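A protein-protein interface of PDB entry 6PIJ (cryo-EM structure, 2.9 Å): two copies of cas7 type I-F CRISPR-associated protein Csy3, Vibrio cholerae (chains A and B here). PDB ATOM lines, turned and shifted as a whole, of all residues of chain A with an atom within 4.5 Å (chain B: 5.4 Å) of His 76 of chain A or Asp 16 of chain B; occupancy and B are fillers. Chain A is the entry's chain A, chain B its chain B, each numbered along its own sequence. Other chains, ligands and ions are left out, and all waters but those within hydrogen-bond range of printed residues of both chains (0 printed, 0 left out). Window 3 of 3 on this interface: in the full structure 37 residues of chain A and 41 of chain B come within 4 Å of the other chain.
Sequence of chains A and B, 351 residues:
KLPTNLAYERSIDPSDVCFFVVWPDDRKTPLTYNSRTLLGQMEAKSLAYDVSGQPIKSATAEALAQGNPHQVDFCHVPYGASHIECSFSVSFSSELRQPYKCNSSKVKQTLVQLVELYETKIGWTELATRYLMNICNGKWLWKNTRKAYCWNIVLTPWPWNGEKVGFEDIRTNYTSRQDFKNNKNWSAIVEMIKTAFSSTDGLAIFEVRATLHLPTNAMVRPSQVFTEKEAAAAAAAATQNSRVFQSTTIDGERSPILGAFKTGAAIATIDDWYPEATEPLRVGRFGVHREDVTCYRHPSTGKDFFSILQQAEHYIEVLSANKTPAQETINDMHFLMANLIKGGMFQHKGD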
ATOM      1  N   LEU A  31     -20.267 -27.914  21.468  1.00  0.00           N
ATOM      2  CA  LEU A  31     -20.798 -27.305  20.218  1.00  0.00           C
ATOM      3  C   LEU A  31     -21.949 -28.177  19.708  1.00  0.00           C
ATOM      4  O   LEU A  31     -21.746 -29.399  19.593  1.00  0.00           O
ATOM      5  CB  LEU A  31     -19.676 -27.198  19.178  1.00  0.00           C
ATOM      6  CG  LEU A  31     -20.068 -26.583  17.833  1.00  0.00           C
ATOM      7  CD1 LEU A  31     -20.552 -25.150  17.998  1.00  0.00           C
ATOM      8  CD2 LEU A  31     -18.903 -26.636  16.860  1.00  0.00           C
ATOM      9  N   ARG A  36     -31.477 -28.757   9.258  1.00  0.00           N
ATOM     10  CA  ARG A  36     -32.015 -27.562   8.558  1.00  0.00           C
ATOM     11  C   ARG A  36     -32.448 -27.988   7.151  1.00  0.00           C
ATOM     12  O   ARG A  36     -31.588 -28.498   6.394  1.00  0.00           O
ATOM     13  CB  ARG A  36     -30.941 -26.471   8.519  1.00  0.00           C
ATOM     14  CG  ARG A  36     -31.439 -25.114   8.043  1.00  0.00           C
ATOM     15  CD  ARG A  36     -30.316 -24.119   7.815  1.00  0.00           C
ATOM     16  NE  ARG A  36     -29.742 -23.628   9.066  1.00  0.00           N
ATOM     17  CZ  ARG A  36     -29.196 -22.423   9.261  1.00  0.00           C
ATOM     18  NH1 ARG A  36     -28.710 -22.114  10.453  1.00  0.00           N
ATOM     19  NH2 ARG A  36     -29.142 -21.523   8.289  1.00  0.00           N
ATOM     20  N   PHE A  74     -26.620 -28.618   9.994  1.00  0.00           N
ATOM     21  CA  PHE A  74     -25.939 -27.296   9.999  1.00  0.00           C
ATOM     22  C   PHE A  74     -25.295 -27.056  11.369  1.00  0.00           C
ATOM     23  O   PHE A  74     -26.031 -26.993  12.376  1.00  0.00           O
ATOM     24  CB  PHE A  74     -26.920 -26.181   9.630  1.00  0.00           C
ATOM     25  CG  PHE A  74     -26.265 -24.944   9.072  1.00  0.00           C
ATOM     26  CD1 PHE A  74     -25.747 -23.971   9.915  1.00  0.00           C
ATOM     27  CD2 PHE A  74     -26.151 -24.760   7.701  1.00  0.00           C
ATOM     28  CE1 PHE A  74     -25.138 -22.836   9.398  1.00  0.00           C
ATOM     29  CE2 PHE A  74     -25.542 -23.624   7.186  1.00  0.00           C
ATOM     30  CZ  PHE A  74     -25.035 -22.665   8.035  1.00  0.00           C
ATOM     31  N   CYS A  75     -23.963 -26.943  11.393  1.00  0.00           N
ATOM     32  CA  CYS A  75     -23.142 -26.576  12.577  1.00  0.00           C
ATOM     33  C   CYS A  75     -22.399 -25.268  12.286  1.00  0.00           C
ATOM     34  O   CYS A  75     -21.809 -25.160  11.193  1.00  0.00           O
ATOM     35  CB  CYS A  75     -22.145 -27.675  12.924  1.00  0.00           C
ATOM     36  SG  CYS A  75     -21.477 -27.524  14.600  1.00  0.00           S
ATOM     37  N   HIS A  76     -22.442 -24.319  13.225  1.00  0.00           N
ATOM     38  CA  HIS A  76     -21.745 -23.006  13.154  1.00  0.00           C
ATOM     39  C   HIS A  76     -21.391 -22.537  14.570  1.00  0.00           C
ATOM     40  O   HIS A  76     -21.931 -23.116  15.535  1.00  0.00           O
ATOM     41  CB  HIS A  76     -22.613 -21.981  12.408  1.00  0.00           C
ATOM     42  CG  HIS A  76     -23.830 -21.561  13.161  1.00  0.00           C
ATOM     43  ND1 HIS A  76     -23.850 -20.431  13.955  1.00  0.00           N
ATOM     44  CD2 HIS A  76     -25.058 -22.115  13.257  1.00  0.00           C
ATOM     45  CE1 HIS A  76     -25.040 -20.305  14.505  1.00  0.00           C
ATOM     46  NE2 HIS A  76     -25.800 -21.326  14.093  1.00  0.00           N
ATOM     47  N   VAL A  77     -20.533 -21.519  14.682  1.00  0.00           N
ATOM     48  CA  VAL A  77     -20.123 -20.916  15.986  1.00  0.00           C
ATOM     49  C   VAL A  77     -21.298 -20.081  16.493  1.00  0.00           C
ATOM     50  O   VAL A  77     -21.787 -19.222  15.764  1.00  0.00           O
ATOM     51  CB  VAL A  77     -18.839 -20.069  15.859  1.00  0.00           C
ATOM     52  CG1 VAL A  77     -18.394 -19.512  17.205  1.00  0.00           C
ATOM     53  CG2 VAL A  77     -17.704 -20.847  15.207  1.00  0.00           C
ATOM     54  N   PRO A  78     -21.799 -20.299  17.735  1.00  0.00           N
ATOM     55  CA  PRO A  78     -22.884 -19.478  18.278  1.00  0.00           C
ATOM     56  C   PRO A  78     -22.448 -18.019  18.477  1.00  0.00           C
ATOM     57  O   PRO A  78     -21.272 -17.788  18.706  1.00  0.00           O
ATOM     58  CB  PRO A  78     -23.213 -20.137  19.627  1.00  0.00           C
ATOM     59  CG  PRO A  78     -21.936 -20.845  20.005  1.00  0.00           C
ATOM     60  CD  PRO A  78     -21.360 -21.330  18.691  1.00  0.00           C
ATOM     61  N   ASN A 217     -20.435 -15.964  13.359  1.00  0.00           N
ATOM     62  CA  ASN A 217     -21.406 -16.996  12.895  1.00  0.00           C
ATOM     63  C   ASN A 217     -20.736 -17.958  11.900  1.00  0.00           C
ATOM     64  O   ASN A 217     -21.464 -18.551  11.075  1.00  0.00           O
ATOM     65  CB  ASN A 217     -22.669 -16.354  12.299  1.00  0.00           C
ATOM     66  CG  ASN A 217     -23.614 -15.783  13.337  1.00  0.00           C
ATOM     67  OD1 ASN A 217     -24.025 -14.630  13.237  1.00  0.00           O
ATOM     68  ND2 ASN A 217     -23.980 -16.585  14.324  1.00  0.00           N
ATOM     69  N   ALA A 218     -19.414 -18.147  11.993  1.00  0.00           N
ATOM     70  CA  ALA A 218     -18.610 -18.947  11.037  1.00  0.00           C
ATOM     71  C   ALA A 218     -19.044 -20.414  11.105  1.00  0.00           C
ATOM     72  O   ALA A 218     -19.383 -20.887  12.209  1.00  0.00           O
ATOM     73  CB  ALA A 218     -17.138 -18.799  11.321  1.00  0.00           C
ATOM     74  N   MET A 219     -19.030 -21.097   9.959  1.00  0.00           N
ATOM     75  CA  MET A 219     -19.542 -22.483   9.794  1.00  0.00           C
ATOM     76  C   MET A 219     -18.447 -23.481  10.194  1.00  0.00           C
ATOM     77  O   MET A 219     -17.285 -23.271   9.789  1.00  0.00           O
ATOM     78  CB  MET A 219     -19.957 -22.727   8.341  1.00  0.00           C
ATOM     79  CG  MET A 219     -20.827 -23.955   8.148  1.00  0.00           C
ATOM     80  SD  MET A 219     -21.146 -24.309   6.399  1.00  0.00           S
ATOM     81  CE  MET A 219     -19.510 -24.802   5.856  1.00  0.00           C
ATOM     82  N   VAL A 220     -18.818 -24.519  10.951  1.00  0.00           N
ATOM     83  CA  VAL A 220     -17.925 -25.636  11.382  1.00  0.00           C
ATOM     84  C   VAL A 220     -18.152 -26.823  10.434  1.00  0.00           C
ATOM     85  O   VAL A 220     -19.320 -27.081  10.079  1.00  0.00           O
ATOM     86  CB  VAL A 220     -18.170 -26.002  12.861  1.00  0.00           C
ATOM     87  CG1 VAL A 220     -17.464 -27.287  13.276  1.00  0.00           C
ATOM     88  CG2 VAL A 220     -17.763 -24.853  13.772  1.00  0.00           C
ATOM     89  N   PRO B  14     -20.806 -16.906   3.125  1.00  0.00           N
ATOM     90  CA  PRO B  14     -21.530 -16.085   4.097  1.00  0.00           C
ATOM     91  C   PRO B  14     -22.001 -16.900   5.313  1.00  0.00           C
ATOM     92  O   PRO B  14     -21.728 -18.089   5.365  1.00  0.00           O
ATOM     93  CB  PRO B  14     -22.715 -15.579   3.268  1.00  0.00           C
ATOM     94  CG  PRO B  14     -23.029 -16.744   2.362  1.00  0.00           C
ATOM     95  CD  PRO B  14     -21.682 -17.353   2.028  1.00  0.00           C
ATOM     96  N   SER B  15     -22.695 -16.242   6.248  1.00  0.00           N
ATOM     97  CA  SER B  15     -23.219 -16.824   7.514  1.00  0.00           C
ATOM     98  C   SER B  15     -24.645 -16.320   7.782  1.00  0.00           C
ATOM     99  O   SER B  15     -25.178 -15.573   6.935  1.00  0.00           O
ATOM    100  CB  SER B  15     -22.292 -16.503   8.661  1.00  0.00           C
ATOM    101  OG  SER B  15     -22.254 -15.106   8.911  1.00  0.00           O
ATOM    102  N   ASP B  16     -25.238 -16.731   8.911  1.00  0.00           N
ATOM    103  CA  ASP B  16     -26.542 -16.224   9.425  1.00  0.00           C
ATOM    104  C   ASP B  16     -26.405 -14.731   9.747  1.00  0.00           C
ATOM    105  O   ASP B  16     -25.304 -14.328  10.180  1.00  0.00           O
ATOM    106  CB  ASP B  16     -26.995 -16.968  10.685  1.00  0.00           C
ATOM    107  CG  ASP B  16     -27.161 -18.471  10.527  1.00  0.00           C
ATOM    108  OD1 ASP B  16     -27.503 -18.912   9.412  1.00  0.00           O
ATOM    109  OD2 ASP B  16     -26.953 -19.190  11.527  1.00  0.00           O
ATOM    110  N   VAL B  17     -27.478 -13.951   9.561  1.00  0.00           N
ATOM    111  CA  VAL B  17     -27.510 -12.486   9.860  1.00  0.00           C
ATOM    112  C   VAL B  17     -28.271 -12.283  11.177  1.00  0.00           C
ATOM    113  O   VAL B  17     -29.513 -12.186  11.141  1.00  0.00           O
ATOM    114  CB  VAL B  17     -28.112 -11.676   8.695  1.00  0.00           C
ATOM    115  CG1 VAL B  17     -28.315 -10.209   9.049  1.00  0.00           C
ATOM    116  CG2 VAL B  17     -27.262 -11.788   7.441  1.00  0.00           C
ATOM    117  N   CYS B  18     -27.542 -12.225  12.295  1.00  0.00           N
ATOM    118  CA  CYS B  18     -28.100 -12.035  13.662  1.00  0.00           C
ATOM    119  C   CYS B  18     -28.641 -10.607  13.801  1.00  0.00           C
ATOM    120  O   CYS B  18     -27.858  -9.657  13.592  1.00  0.00           O
ATOM    121  CB  CYS B  18     -27.056 -12.315  14.739  1.00  0.00           C
ATOM    122  SG  CYS B  18     -26.666 -14.075  14.918  1.00  0.00           S
ATOM    123  N   SER B  87     -25.797  -8.192  11.810  1.00  0.00           N
ATOM    124  CA  SER B  87     -24.358  -8.575  11.799  1.00  0.00           C
ATOM    125  C   SER B  87     -24.165  -9.966  11.181  1.00  0.00           C
ATOM    126  O   SER B  87     -24.909 -10.892  11.570  1.00  0.00           O
ATOM    127  CB  SER B  87     -23.776  -8.512  13.188  1.00  0.00           C
ATOM    128  OG  SER B  87     -24.415  -9.440  14.052  1.00  0.00           O
ATOM    129  N   PHE B  88     -23.200 -10.095  10.261  1.00  0.00           N
ATOM    130  CA  PHE B  88     -22.730 -11.380   9.674  1.00  0.00           C
ATOM    131  C   PHE B  88     -21.313 -11.211   9.103  1.00  0.00           C
ATOM    132  O   PHE B  88     -20.789 -10.074   9.091  1.00  0.00           O
ATOM    133  CB  PHE B  88     -23.721 -11.883   8.619  1.00  0.00           C
ATOM    134  CG  PHE B  88     -23.532 -11.324   7.232  1.00  0.00           C
ATOM    135  CD1 PHE B  88     -23.722  -9.973   6.976  1.00  0.00           C
ATOM    136  CD2 PHE B  88     -23.176 -12.149   6.175  1.00  0.00           C
ATOM    137  CE1 PHE B  88     -23.553  -9.462   5.698  1.00  0.00           C
ATOM    138  CE2 PHE B  88     -23.012 -11.637   4.896  1.00  0.00           C
ATOM    139  CZ  PHE B  88     -23.194 -10.293   4.661  1.00  0.00           C
ATOM    140  N   SER B  89     -20.721 -12.318   8.637  1.00  0.00           N
ATOM    141  CA  SER B  89     -19.338 -12.401   8.093  1.00  0.00           C
ATOM    142  C   SER B  89     -19.342 -13.083   6.718  1.00  0.00           C
ATOM    143  O   SER B  89     -20.122 -14.039   6.539  1.00  0.00           O
ATOM    144  CB  SER B  89     -18.428 -13.122   9.056  1.00  0.00           C
ATOM    145  OG  SER B  89     -18.640 -14.526   9.008  1.00  0.00           O
ATOM    146  N   THR B 248     -32.240 -18.800  15.732  1.00  0.00           N
ATOM    147  CA  THR B 248     -31.097 -19.242  16.582  1.00  0.00           C
ATOM    148  C   THR B 248     -31.307 -18.737  18.014  1.00  0.00           C
ATOM    149  O   THR B 248     -32.218 -17.905  18.224  1.00  0.00           O
ATOM    150  CB  THR B 248     -29.738 -18.764  16.052  1.00  0.00           C
ATOM    151  OG1 THR B 248     -29.797 -17.352  15.850  1.00  0.00           O
ATOM    152  CG2 THR B 248     -29.313 -19.469  14.781  1.00  0.00           C
ATOM    153  N   ILE B 257     -33.095 -14.921  12.020  1.00  0.00           N
ATOM    154  CA  ILE B 257     -31.671 -15.076  11.573  1.00  0.00           C
ATOM    155  C   ILE B 257     -31.425 -14.649  10.111  1.00  0.00           C
ATOM    156  O   ILE B 257     -30.241 -14.393   9.790  1.00  0.00           O
ATOM    157  CB  ILE B 257     -31.199 -16.522  11.837  1.00  0.00           C
ATOM    158  CG1 ILE B 257     -31.862 -17.558  10.926  1.00  0.00           C
ATOM    159  CG2 ILE B 257     -31.406 -16.877  13.299  1.00  0.00           C
ATOM    160  CD1 ILE B 257     -31.042 -18.814  10.739  1.00  0.00           C
ATOM    161  N   GLY B 259     -31.268 -16.414   7.392  1.00  0.00           N
ATOM    162  CA  GLY B 259     -30.629 -17.487   6.600  1.00  0.00           C
ATOM    163  C   GLY B 259     -29.128 -17.321   6.396  1.00  0.00           C
ATOM    164  O   GLY B 259     -28.619 -16.191   6.524  1.00  0.00           O
ATOM    165  N   ALA B 260     -28.447 -18.428   6.083  1.00  0.00           N
ATOM    166  CA  ALA B 260     -27.036 -18.485   5.626  1.00  0.00           C
ATOM    167  C   ALA B 260     -26.994 -18.586   4.096  1.00  0.00           C
ATOM    168  O   ALA B 260     -26.166 -17.888   3.480  1.00  0.00           O
ATOM    169  CB  ALA B 260     -26.326 -19.654   6.263  1.00  0.00           C
ATOM    170  N   THR B 263     -28.350 -15.308   2.192  1.00  0.00           N
ATOM    171  CA  THR B 263     -27.360 -14.197   2.179  1.00  0.00           C
ATOM    172  C   THR B 263     -26.297 -14.451   1.100  1.00  0.00           C
ATOM    173  O   THR B 263     -25.745 -13.459   0.590  1.00  0.00           O
ATOM    174  CB  THR B 263     -26.766 -13.986   3.577  1.00  0.00           C
ATOM    175  OG1 THR B 263     -26.144 -15.199   3.998  1.00  0.00           O
ATOM    176  CG2 THR B 263     -27.813 -13.577   4.589  1.00  0.00           C
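No position is printed for both chains.
Of the 7 pairs that touch across the chains among the printed residues, none has its exchanged pair printed and touching as well.
Of chain A, only Arg 36, His 76 and Asn 217 come within 4 Å of Asp 16 of chain B.
Of the printed residues of chain A, Ser 15 of chain B touches Asn 217 (3.3 Å).
Printed residues of chain A within 4 Å of Cys 18 of chain B: Asn 217.
Of the printed residues of chain B, Arg 36 of chain A touches Asp 16 and Ala 260.
Of the printed residues of chain B, Phe 74 of chain A touches Ala 260.
Printed residues of chain B within 4 Å of Asn 217 of chain A: Ser 15 (3.3 Å), Asp 16 (3.3 Å) and Cys 18 (3.2 Å).
The nearest printed residue of chain A that does not touch Asp 16 of chain B is Phe 74 of chain A (4.6 Å).
Ala 260 of chain B touches Arg 36 of chain A.
Phe 74 of chain A touches Ala 260 of chain B.
His 76 of chain A touches Asp 16 of chain B.
Asn 217 of chain A touches Ser 15 of chain B.
NH2 of Arg 36 of chain A is in salt-bridge range of OD1 of Asp 16 of chain B (3.3 Å).
The side-chain amide oxygen of Asn 217 of chain A is in hydrogen-bond range of the side-chain sulfur of Cys 18 of chain B (3.2 Å).
The backbone carbonyl oxygen (O) of Asp 16 of chain B sits close to the side-chain amide oxygen (OD1) of Asn 217 of chain A, 3.3 Å away.
Hydrophobic or aromatic side chains of chain A that line the printed part of chain B: Phe 74 and His 76.
Along chain A the printed residues that touch a printed residue of chain B span positions 36 to 217.
Hydrophobic or aromatic side chains of chain B that line the printed part of chain A: Ala 260.
Among the printed residues, 7 pairs touch across the chains.
Among the printed residues, Asp or Glu carboxylates within 4 Å of a Lys or Arg side-chain nitrogen of the other chain: Arg 36 of chain A with Asp 16 of chain B.
The side-chain hydroxyl (OG1) of Thr 263 of chain B sits at hydrogen-bond distance from the backbone carbonyl oxygen (O) of Ser 15 of chain B (3.1 Å).
O of Ala 260 of chain B lies within hydrogen-bond range of OG1 of Thr 263 of chain B, at 2.7 Å.
The side-chain carboxylate (OD1) of Asp 16 of chain B sits close to the backbone NH (N) of Ala 260 of chain B, at 3.5 Å.
N of Cys 18 of chain B lies within hydrogen-bond range of O of Ser 87 of chain B (3.0 Å).
The side-chain hydroxyl (OG) of Ser 15 of chain B lies within hydrogen-bond range of the backbone NH (N) of Ser 89 of chain B (3.2 Å).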
